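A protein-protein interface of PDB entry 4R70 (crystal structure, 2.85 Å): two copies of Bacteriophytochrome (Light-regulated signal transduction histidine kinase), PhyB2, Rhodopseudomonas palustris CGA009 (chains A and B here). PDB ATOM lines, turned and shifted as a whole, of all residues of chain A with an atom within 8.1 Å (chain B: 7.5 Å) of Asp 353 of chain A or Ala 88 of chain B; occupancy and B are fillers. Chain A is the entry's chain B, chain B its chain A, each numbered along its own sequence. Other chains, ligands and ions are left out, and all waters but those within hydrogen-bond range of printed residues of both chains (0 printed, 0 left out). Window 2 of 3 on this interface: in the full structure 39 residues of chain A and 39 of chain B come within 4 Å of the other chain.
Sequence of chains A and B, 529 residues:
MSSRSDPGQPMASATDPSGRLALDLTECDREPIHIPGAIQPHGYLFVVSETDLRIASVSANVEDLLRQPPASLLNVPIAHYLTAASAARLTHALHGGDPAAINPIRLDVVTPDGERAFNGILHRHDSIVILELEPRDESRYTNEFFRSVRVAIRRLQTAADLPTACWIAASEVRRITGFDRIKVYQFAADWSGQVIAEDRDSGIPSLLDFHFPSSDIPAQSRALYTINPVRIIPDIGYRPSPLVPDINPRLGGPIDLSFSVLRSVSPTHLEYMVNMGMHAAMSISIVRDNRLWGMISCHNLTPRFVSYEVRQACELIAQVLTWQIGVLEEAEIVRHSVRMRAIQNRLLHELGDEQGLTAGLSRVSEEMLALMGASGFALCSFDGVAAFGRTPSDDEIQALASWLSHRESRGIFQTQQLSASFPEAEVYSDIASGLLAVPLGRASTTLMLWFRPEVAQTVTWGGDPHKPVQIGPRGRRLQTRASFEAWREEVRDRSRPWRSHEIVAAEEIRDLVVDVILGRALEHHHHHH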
ATOM      1  N   ARG A 346     -10.391 -28.873  15.262  1.00  0.00           N
ATOM      2  CA  ARG A 346     -10.878 -28.939  16.630  1.00  0.00           C
ATOM      3  C   ARG A 346     -11.537 -27.651  17.042  1.00  0.00           C
ATOM      4  O   ARG A 346     -12.754 -27.591  17.333  1.00  0.00           O
ATOM      5  CB  ARG A 346      -9.728 -29.265  17.594  1.00  0.00           C
ATOM      6  CG  ARG A 346     -10.142 -29.859  18.958  1.00  0.00           C
ATOM      7  CD  ARG A 346      -8.921 -30.529  19.601  1.00  0.00           C
ATOM      8  NE  ARG A 346      -8.495 -31.738  18.859  1.00  0.00           N
ATOM      9  CZ  ARG A 346      -7.246 -32.025  18.449  1.00  0.00           C
ATOM     10  NH1 ARG A 346      -6.236 -31.199  18.689  1.00  0.00           N
ATOM     11  NH2 ARG A 346      -6.987 -33.156  17.787  1.00  0.00           N
ATOM     12  N   LEU A 347     -10.730 -26.600  16.914  1.00  0.00           N
ATOM     13  CA  LEU A 347     -11.022 -25.265  17.407  1.00  0.00           C
ATOM     14  C   LEU A 347     -12.344 -24.994  16.829  1.00  0.00           C
ATOM     15  O   LEU A 347     -13.237 -24.535  17.497  1.00  0.00           O
ATOM     16  CB  LEU A 347     -10.098 -24.324  16.694  1.00  0.00           C
ATOM     17  CG  LEU A 347      -8.670 -24.113  17.199  1.00  0.00           C
ATOM     18  CD1 LEU A 347      -7.900 -23.401  16.118  1.00  0.00           C
ATOM     19  CD2 LEU A 347      -8.618 -23.297  18.436  1.00  0.00           C
ATOM     20  N   LEU A 348     -12.453 -25.301  15.551  1.00  0.00           N
ATOM     21  CA  LEU A 348     -13.683 -25.042  14.822  1.00  0.00           C
ATOM     22  C   LEU A 348     -14.843 -25.652  15.569  1.00  0.00           C
ATOM     23  O   LEU A 348     -15.759 -24.975  15.965  1.00  0.00           O
ATOM     24  CB  LEU A 348     -13.602 -25.628  13.411  1.00  0.00           C
ATOM     25  CG  LEU A 348     -14.748 -25.320  12.447  1.00  0.00           C
ATOM     26  CD1 LEU A 348     -14.439 -25.781  10.974  1.00  0.00           C
ATOM     27  CD2 LEU A 348     -16.120 -25.822  12.830  1.00  0.00           C
ATOM     28  N   HIS A 349     -14.811 -26.956  15.714  1.00  0.00           N
ATOM     29  CA  HIS A 349     -15.946 -27.633  16.219  1.00  0.00           C
ATOM     30  C   HIS A 349     -16.139 -27.374  17.684  1.00  0.00           C
ATOM     31  O   HIS A 349     -17.271 -27.303  18.173  1.00  0.00           O
ATOM     32  CB  HIS A 349     -15.861 -29.084  15.837  1.00  0.00           C
ATOM     33  CG  HIS A 349     -15.997 -29.272  14.359  1.00  0.00           C
ATOM     34  ND1 HIS A 349     -17.126 -28.918  13.672  1.00  0.00           N
ATOM     35  CD2 HIS A 349     -15.123 -29.777  13.439  1.00  0.00           C
ATOM     36  CE1 HIS A 349     -16.971 -29.196  12.394  1.00  0.00           C
ATOM     37  NE2 HIS A 349     -15.776 -29.728  12.219  1.00  0.00           N
ATOM     38  N   GLU A 350     -15.033 -27.226  18.389  1.00  0.00           N
ATOM     39  CA  GLU A 350     -15.169 -27.101  19.833  1.00  0.00           C
ATOM     40  C   GLU A 350     -15.743 -25.738  20.220  1.00  0.00           C
ATOM     41  O   GLU A 350     -16.298 -25.580  21.298  1.00  0.00           O
ATOM     42  CB  GLU A 350     -13.873 -27.425  20.559  1.00  0.00           C
ATOM     43  CG  GLU A 350     -14.049 -27.692  22.037  1.00  0.00           C
ATOM     44  CD  GLU A 350     -14.374 -29.160  22.340  1.00  0.00           C
ATOM     45  OE1 GLU A 350     -15.234 -29.742  21.643  1.00  0.00           O
ATOM     46  OE2 GLU A 350     -13.750 -29.736  23.273  1.00  0.00           O
ATOM     47  N   LEU A 351     -15.540 -24.735  19.376  1.00  0.00           N
ATOM     48  CA  LEU A 351     -16.208 -23.437  19.567  1.00  0.00           C
ATOM     49  C   LEU A 351     -17.583 -23.531  18.985  1.00  0.00           C
ATOM     50  O   LEU A 351     -18.523 -22.829  19.391  1.00  0.00           O
ATOM     51  CB  LEU A 351     -15.473 -22.290  18.913  1.00  0.00           C
ATOM     52  CG  LEU A 351     -14.424 -21.696  19.828  1.00  0.00           C
ATOM     53  CD1 LEU A 351     -13.059 -22.269  19.490  1.00  0.00           C
ATOM     54  CD2 LEU A 351     -14.416 -20.212  19.698  1.00  0.00           C
ATOM     55  N   GLY A 352     -17.661 -24.436  18.020  1.00  0.00           N
ATOM     56  CA  GLY A 352     -18.792 -24.572  17.134  1.00  0.00           C
ATOM     57  C   GLY A 352     -20.139 -24.641  17.805  1.00  0.00           C
ATOM     58  O   GLY A 352     -21.116 -23.979  17.412  1.00  0.00           O
ATOM     59  N   ASP A 353     -20.201 -25.458  18.835  1.00  0.00           N
ATOM     60  CA  ASP A 353     -21.501 -25.921  19.289  1.00  0.00           C
ATOM     61  C   ASP A 353     -21.927 -25.388  20.671  1.00  0.00           C
ATOM     62  O   ASP A 353     -23.127 -25.272  21.008  1.00  0.00           O
ATOM     63  CB  ASP A 353     -21.485 -27.448  19.171  1.00  0.00           C
ATOM     64  CG  ASP A 353     -21.181 -27.900  17.732  1.00  0.00           C
ATOM     65  OD1 ASP A 353     -20.008 -28.237  17.413  1.00  0.00           O
ATOM     66  OD2 ASP A 353     -22.118 -27.837  16.902  1.00  0.00           O
ATOM     67  N   GLU A 354     -20.922 -24.956  21.415  1.00  0.00           N
ATOM     68  CA  GLU A 354     -21.116 -24.407  22.739  1.00  0.00           C
ATOM     69  C   GLU A 354     -21.879 -23.069  22.706  1.00  0.00           C
ATOM     70  O   GLU A 354     -21.791 -22.322  21.729  1.00  0.00           O
ATOM     71  CB  GLU A 354     -19.744 -24.286  23.435  1.00  0.00           C
ATOM     72  CG  GLU A 354     -19.775 -24.452  24.946  1.00  0.00           C
ATOM     73  CD  GLU A 354     -20.430 -23.251  25.621  1.00  0.00           C
ATOM     74  OE1 GLU A 354     -20.116 -22.126  25.199  1.00  0.00           O
ATOM     75  OE2 GLU A 354     -21.277 -23.418  26.538  1.00  0.00           O
ATOM     76  N   GLN A 355     -22.670 -22.823  23.752  1.00  0.00           N
ATOM     77  CA  GLN A 355     -23.548 -21.645  23.851  1.00  0.00           C
ATOM     78  C   GLN A 355     -22.780 -20.361  24.257  1.00  0.00           C
ATOM     79  O   GLN A 355     -23.380 -19.295  24.445  1.00  0.00           O
ATOM     80  CB  GLN A 355     -24.707 -21.915  24.838  1.00  0.00           C
ATOM     81  CG  GLN A 355     -25.900 -20.912  24.815  1.00  0.00           C
ATOM     82  CD  GLN A 355     -26.170 -20.252  26.192  1.00  0.00           C
ATOM     83  OE1 GLN A 355     -26.083 -20.904  27.249  1.00  0.00           O
ATOM     84  NE2 GLN A 355     -26.478 -18.957  26.178  1.00  0.00           N
ATOM     85  N   GLY A 356     -21.460 -20.454  24.362  1.00  0.00           N
ATOM     86  CA  GLY A 356     -20.633 -19.265  24.496  1.00  0.00           C
ATOM     87  C   GLY A 356     -19.417 -19.374  23.604  1.00  0.00           C
ATOM     88  O   GLY A 356     -18.952 -20.469  23.301  1.00  0.00           O
ATOM     89  N   GLY A 360     -15.867 -21.628  24.405  1.00  0.00           N
ATOM     90  CA  GLY A 360     -15.331 -22.457  23.344  1.00  0.00           C
ATOM     91  C   GLY A 360     -13.831 -22.302  23.244  1.00  0.00           C
ATOM     92  O   GLY A 360     -13.086 -23.192  22.778  1.00  0.00           O
ATOM     93  N   ARG A 520     -22.185 -15.701  14.186  1.00  0.00           N
ATOM     94  CA  ARG A 520     -23.214 -15.640  15.204  1.00  0.00           C
ATOM     95  C   ARG A 520     -23.526 -14.207  15.563  1.00  0.00           C
ATOM     96  O   ARG A 520     -22.755 -13.571  16.260  1.00  0.00           O
ATOM     97  CB  ARG A 520     -22.756 -16.390  16.460  1.00  0.00           C
ATOM     98  CG  ARG A 520     -21.286 -16.257  16.773  1.00  0.00           C
ATOM     99  CD  ARG A 520     -20.999 -16.166  18.278  1.00  0.00           C
ATOM    100  NE  ARG A 520     -21.418 -17.346  19.050  1.00  0.00           N
ATOM    101  CZ  ARG A 520     -20.596 -18.303  19.490  1.00  0.00           C
ATOM    102  NH1 ARG A 520     -19.297 -18.241  19.230  1.00  0.00           N
ATOM    103  NH2 ARG A 520     -21.077 -19.328  20.190  1.00  0.00           N
ATOM    104  N   ALA B  79     -30.913 -35.724  12.129  1.00  0.00           N
ATOM    105  CA  ALA B  79     -30.540 -35.469  13.512  1.00  0.00           C
ATOM    106  C   ALA B  79     -31.230 -36.428  14.517  1.00  0.00           C
ATOM    107  O   ALA B  79     -30.755 -36.626  15.639  1.00  0.00           O
ATOM    108  CB  ALA B  79     -30.797 -33.995  13.865  1.00  0.00           C
ATOM    109  N   LEU B  82     -28.905 -38.772  15.431  1.00  0.00           N
ATOM    110  CA  LEU B  82     -27.739 -38.257  16.103  1.00  0.00           C
ATOM    111  C   LEU B  82     -27.954 -37.811  17.565  1.00  0.00           C
ATOM    112  O   LEU B  82     -29.051 -37.408  17.964  1.00  0.00           O
ATOM    113  CB  LEU B  82     -27.188 -37.090  15.308  1.00  0.00           C
ATOM    114  CG  LEU B  82     -25.961 -37.492  14.486  1.00  0.00           C
ATOM    115  CD1 LEU B  82     -26.056 -38.883  13.822  1.00  0.00           C
ATOM    116  CD2 LEU B  82     -25.543 -36.361  13.551  1.00  0.00           C
ATOM    117  N   THR B  83     -26.895 -37.938  18.359  1.00  0.00           N
ATOM    118  CA  THR B  83     -26.821 -37.345  19.686  1.00  0.00           C
ATOM    119  C   THR B  83     -26.967 -35.813  19.667  1.00  0.00           C
ATOM    120  O   THR B  83     -26.712 -35.164  18.642  1.00  0.00           O
ATOM    121  CB  THR B  83     -25.486 -37.663  20.308  1.00  0.00           C
ATOM    122  OG1 THR B  83     -24.484 -36.776  19.804  1.00  0.00           O
ATOM    123  CG2 THR B  83     -25.157 -39.135  20.064  1.00  0.00           C
ATOM    124  N   ALA B  84     -27.386 -35.255  20.807  1.00  0.00           N
ATOM    125  CA  ALA B  84     -27.668 -33.822  20.952  1.00  0.00           C
ATOM    126  C   ALA B  84     -26.518 -33.057  20.383  1.00  0.00           C
ATOM    127  O   ALA B  84     -26.701 -32.151  19.586  1.00  0.00           O
ATOM    128  CB  ALA B  84     -27.853 -33.440  22.436  1.00  0.00           C
ATOM    129  N   ALA B  85     -25.327 -33.443  20.803  1.00  0.00           N
ATOM    130  CA  ALA B  85     -24.111 -32.782  20.375  1.00  0.00           C
ATOM    131  C   ALA B  85     -23.789 -33.067  18.889  1.00  0.00           C
ATOM    132  O   ALA B  85     -23.397 -32.143  18.161  1.00  0.00           O
ATOM    133  CB  ALA B  85     -22.948 -33.189  21.301  1.00  0.00           C
ATOM    134  N   SER B  86     -23.925 -34.314  18.431  1.00  0.00           N
ATOM    135  CA  SER B  86     -23.545 -34.630  17.042  1.00  0.00           C
ATOM    136  C   SER B  86     -24.359 -33.864  16.027  1.00  0.00           C
ATOM    137  O   SER B  86     -23.815 -33.274  15.108  1.00  0.00           O
ATOM    138  CB  SER B  86     -23.631 -36.119  16.747  1.00  0.00           C
ATOM    139  OG  SER B  86     -22.857 -36.865  17.661  1.00  0.00           O
ATOM    140  N   ALA B  87     -25.673 -33.920  16.201  1.00  0.00           N
ATOM    141  CA  ALA B  87     -26.633 -33.255  15.355  1.00  0.00           C
ATOM    142  C   ALA B  87     -26.301 -31.803  15.213  1.00  0.00           C
ATOM    143  O   ALA B  87     -26.189 -31.286  14.123  1.00  0.00           O
ATOM    144  CB  ALA B  87     -27.982 -33.396  15.958  1.00  0.00           C
ATOM    145  N   ALA B  88     -26.065 -31.146  16.329  1.00  0.00           N
ATOM    146  CA  ALA B  88     -25.693 -29.752  16.285  1.00  0.00           C
ATOM    147  C   ALA B  88     -24.321 -29.570  15.641  1.00  0.00           C
ATOM    148  O   ALA B  88     -24.131 -28.626  14.882  1.00  0.00           O
ATOM    149  CB  ALA B  88     -25.689 -29.190  17.661  1.00  0.00           C
ATOM    150  N   ARG B  89     -23.376 -30.464  15.937  1.00  0.00           N
ATOM    151  CA  ARG B  89     -22.016 -30.335  15.425  1.00  0.00           C
ATOM    152  C   ARG B  89     -22.156 -30.377  13.941  1.00  0.00           C
ATOM    153  O   ARG B  89     -21.480 -29.652  13.231  1.00  0.00           O
ATOM    154  CB  ARG B  89     -21.118 -31.482  15.916  1.00  0.00           C
ATOM    155  CG  ARG B  89     -19.613 -31.149  16.003  1.00  0.00           C
ATOM    156  CD  ARG B  89     -18.941 -31.963  17.106  1.00  0.00           C
ATOM    157  NE  ARG B  89     -19.356 -33.357  17.052  1.00  0.00           N
ATOM    158  CZ  ARG B  89     -20.089 -33.969  17.981  1.00  0.00           C
ATOM    159  NH1 ARG B  89     -20.473 -33.311  19.063  1.00  0.00           N
ATOM    160  NH2 ARG B  89     -20.420 -35.254  17.836  1.00  0.00           N
ATOM    161  N   LEU B  90     -23.073 -31.219  13.486  1.00  0.00           N
ATOM    162  CA  LEU B  90     -23.348 -31.374  12.078  1.00  0.00           C
ATOM    163  C   LEU B  90     -24.025 -30.131  11.573  1.00  0.00           C
ATOM    164  O   LEU B  90     -23.495 -29.449  10.702  1.00  0.00           O
ATOM    165  CB  LEU B  90     -24.264 -32.550  11.847  1.00  0.00           C
ATOM    166  CG  LEU B  90     -24.518 -32.739  10.365  1.00  0.00           C
ATOM    167  CD1 LEU B  90     -23.199 -33.020   9.731  1.00  0.00           C
ATOM    168  CD2 LEU B  90     -25.474 -33.880  10.133  1.00  0.00           C
ATOM    169  N   THR B  91     -25.221 -29.880  12.103  1.00  0.00           N
ATOM    170  CA  THR B  91     -25.930 -28.631  11.857  1.00  0.00           C
ATOM    171  C   THR B  91     -25.003 -27.446  11.918  1.00  0.00           C
ATOM    172  O   THR B  91     -24.929 -26.714  10.959  1.00  0.00           O
ATOM    173  CB  THR B  91     -27.055 -28.393  12.834  1.00  0.00           C
ATOM    174  OG1 THR B  91     -28.227 -29.063  12.351  1.00  0.00           O
ATOM    175  CG2 THR B  91     -27.363 -26.903  12.916  1.00  0.00           C
ATOM    176  N   HIS B  92     -24.270 -27.236  13.009  1.00  0.00           N
ATOM    177  CA  HIS B  92     -23.381 -26.082  13.009  1.00  0.00           C
ATOM    178  C   HIS B  92     -22.406 -26.208  11.863  1.00  0.00           C
ATOM    179  O   HIS B  92     -21.877 -25.206  11.401  1.00  0.00           O
ATOM    180  CB  HIS B  92     -22.629 -25.853  14.301  1.00  0.00           C
ATOM    181  CG  HIS B  92     -21.736 -24.646  14.235  1.00  0.00           C
ATOM    182  ND1 HIS B  92     -20.518 -24.659  13.578  1.00  0.00           N
ATOM    183  CD2 HIS B  92     -21.910 -23.386  14.678  1.00  0.00           C
ATOM    184  CE1 HIS B  92     -19.970 -23.477  13.639  1.00  0.00           C
ATOM    185  NE2 HIS B  92     -20.791 -22.666  14.317  1.00  0.00           N
ATOM    186  N   ALA B  93     -22.050 -27.427  11.482  1.00  0.00           N
ATOM    187  CA  ALA B  93     -21.169 -27.580  10.329  1.00  0.00           C
ATOM    188  C   ALA B  93     -21.897 -27.369   8.977  1.00  0.00           C
ATOM    189  O   ALA B  93     -21.232 -27.040   7.990  1.00  0.00           O
ATOM    190  CB  ALA B  93     -20.444 -28.882  10.360  1.00  0.00           C
ATOM    191  N   LEU B  94     -23.227 -27.573   8.934  1.00  0.00           N
ATOM    192  CA  LEU B  94     -24.060 -27.355   7.723  1.00  0.00           C
ATOM    193  C   LEU B  94     -23.862 -25.962   7.171  1.00  0.00           C
ATOM    194  O   LEU B  94     -23.860 -25.809   5.973  1.00  0.00           O
ATOM    195  CB  LEU B  94     -25.547 -27.666   7.956  1.00  0.00           C
ATOM    196  CG  LEU B  94     -26.716 -26.647   7.981  1.00  0.00           C
ATOM    197  CD1 LEU B  94     -27.608 -26.726   6.735  1.00  0.00           C
ATOM    198  CD2 LEU B  94     -27.616 -26.736   9.239  1.00  0.00           C
ATOM    199  N   ILE B 105     -15.979 -34.584  10.589  1.00  0.00           N
ATOM    200  CA  ILE B 105     -16.763 -34.208  11.746  1.00  0.00           C
ATOM    201  C   ILE B 105     -17.049 -35.409  12.616  1.00  0.00           C
ATOM    202  O   ILE B 105     -17.519 -36.438  12.147  1.00  0.00           O
ATOM    203  CB  ILE B 105     -18.107 -33.628  11.309  1.00  0.00           C
ATOM    204  CG1 ILE B 105     -17.895 -32.364  10.487  1.00  0.00           C
ATOM    205  CG2 ILE B 105     -18.922 -33.249  12.524  1.00  0.00           C
ATOM    206  CD1 ILE B 105     -19.107 -31.943   9.774  1.00  0.00           C
ATOM    207  N   LEU B 107     -19.112 -37.670  14.287  1.00  0.00           N
ATOM    208  CA  LEU B 107     -20.541 -37.889  14.444  1.00  0.00           C
ATOM    209  C   LEU B 107     -20.681 -39.054  15.376  1.00  0.00           C
ATOM    210  O   LEU B 107     -19.864 -39.970  15.343  1.00  0.00           O
ATOM    211  CB  LEU B 107     -21.163 -38.243  13.121  1.00  0.00           C
ATOM    212  CG  LEU B 107     -21.010 -37.132  12.118  1.00  0.00           C
ATOM    213  CD1 LEU B 107     -21.501 -37.664  10.805  1.00  0.00           C
ATOM    214  CD2 LEU B 107     -21.781 -35.893  12.573  1.00  0.00           C
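His 349 of chain A touches Ile 105 of chain B.
Asp 353 of chain A touches His 92 of chain B.
Of the 13 printed residues of chain A, 3 touch a printed residue of chain B.
Hydrophobic or aromatic side chains of chain A within 4 Å of the printed part of chain B: His 349.
Of the 16 printed residues of chain B, 4 touch a printed residue of chain A.
Hydrophobic or aromatic side chains of chain B that line the printed part of chain A: Ala 88, His 92 and Ile 105.
Among the printed residues, 5 pairs touch across the chains.
Among the printed residues, no Asp or Glu carboxylate lies within 4 Å of a Lys or Arg side-chain nitrogen of the other chain.
O of Ala 88 of chain B sits close to OD2 of Asp 353 of chain A, at 3.0 Å.
A ring nitrogen (NE2) of His 92 of chain B sits close to the backbone carbonyl oxygen of Gly 352 of chain A (3.4 Å).
N of Arg 89 of chain B lies close to OD2 of Asp 353 of chain A (3.1 Å).
Asp 353 of chain A touches just these residues of chain B: Ala 88 (3.0 Å), Arg 89 (2.9 Å) and His 92 (3.3 Å).
Ala 88 of chain B touches just one residue of chain A: Asp 353.
Gly 352 of chain A touches one residue of chain B.
Printed residues of chain A within 4 Å of Ile 105 of chain B: His 349 (3.8 Å).
Of the printed residues of chain A, His 92 of chain B touches Gly 352 and Asp 353.
Printed residues of chain B within 4 Å of His 349 of chain A: Ile 105 (3.8 Å).
Ala 84 of chain B touches none of the printed residues of chain A.
No position is printed for both chains.
The backbone carbonyl oxygen (O) of Ala 85 of chain B sits close to the guanidinium group (NH1) of Arg 89 of chain B (3.3 Å).
The side-chain hydroxyl (OG) of Ser 86 of chain B is in hydrogen-bond range of the guanidinium group (NH2) of Arg 89 of chain B.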
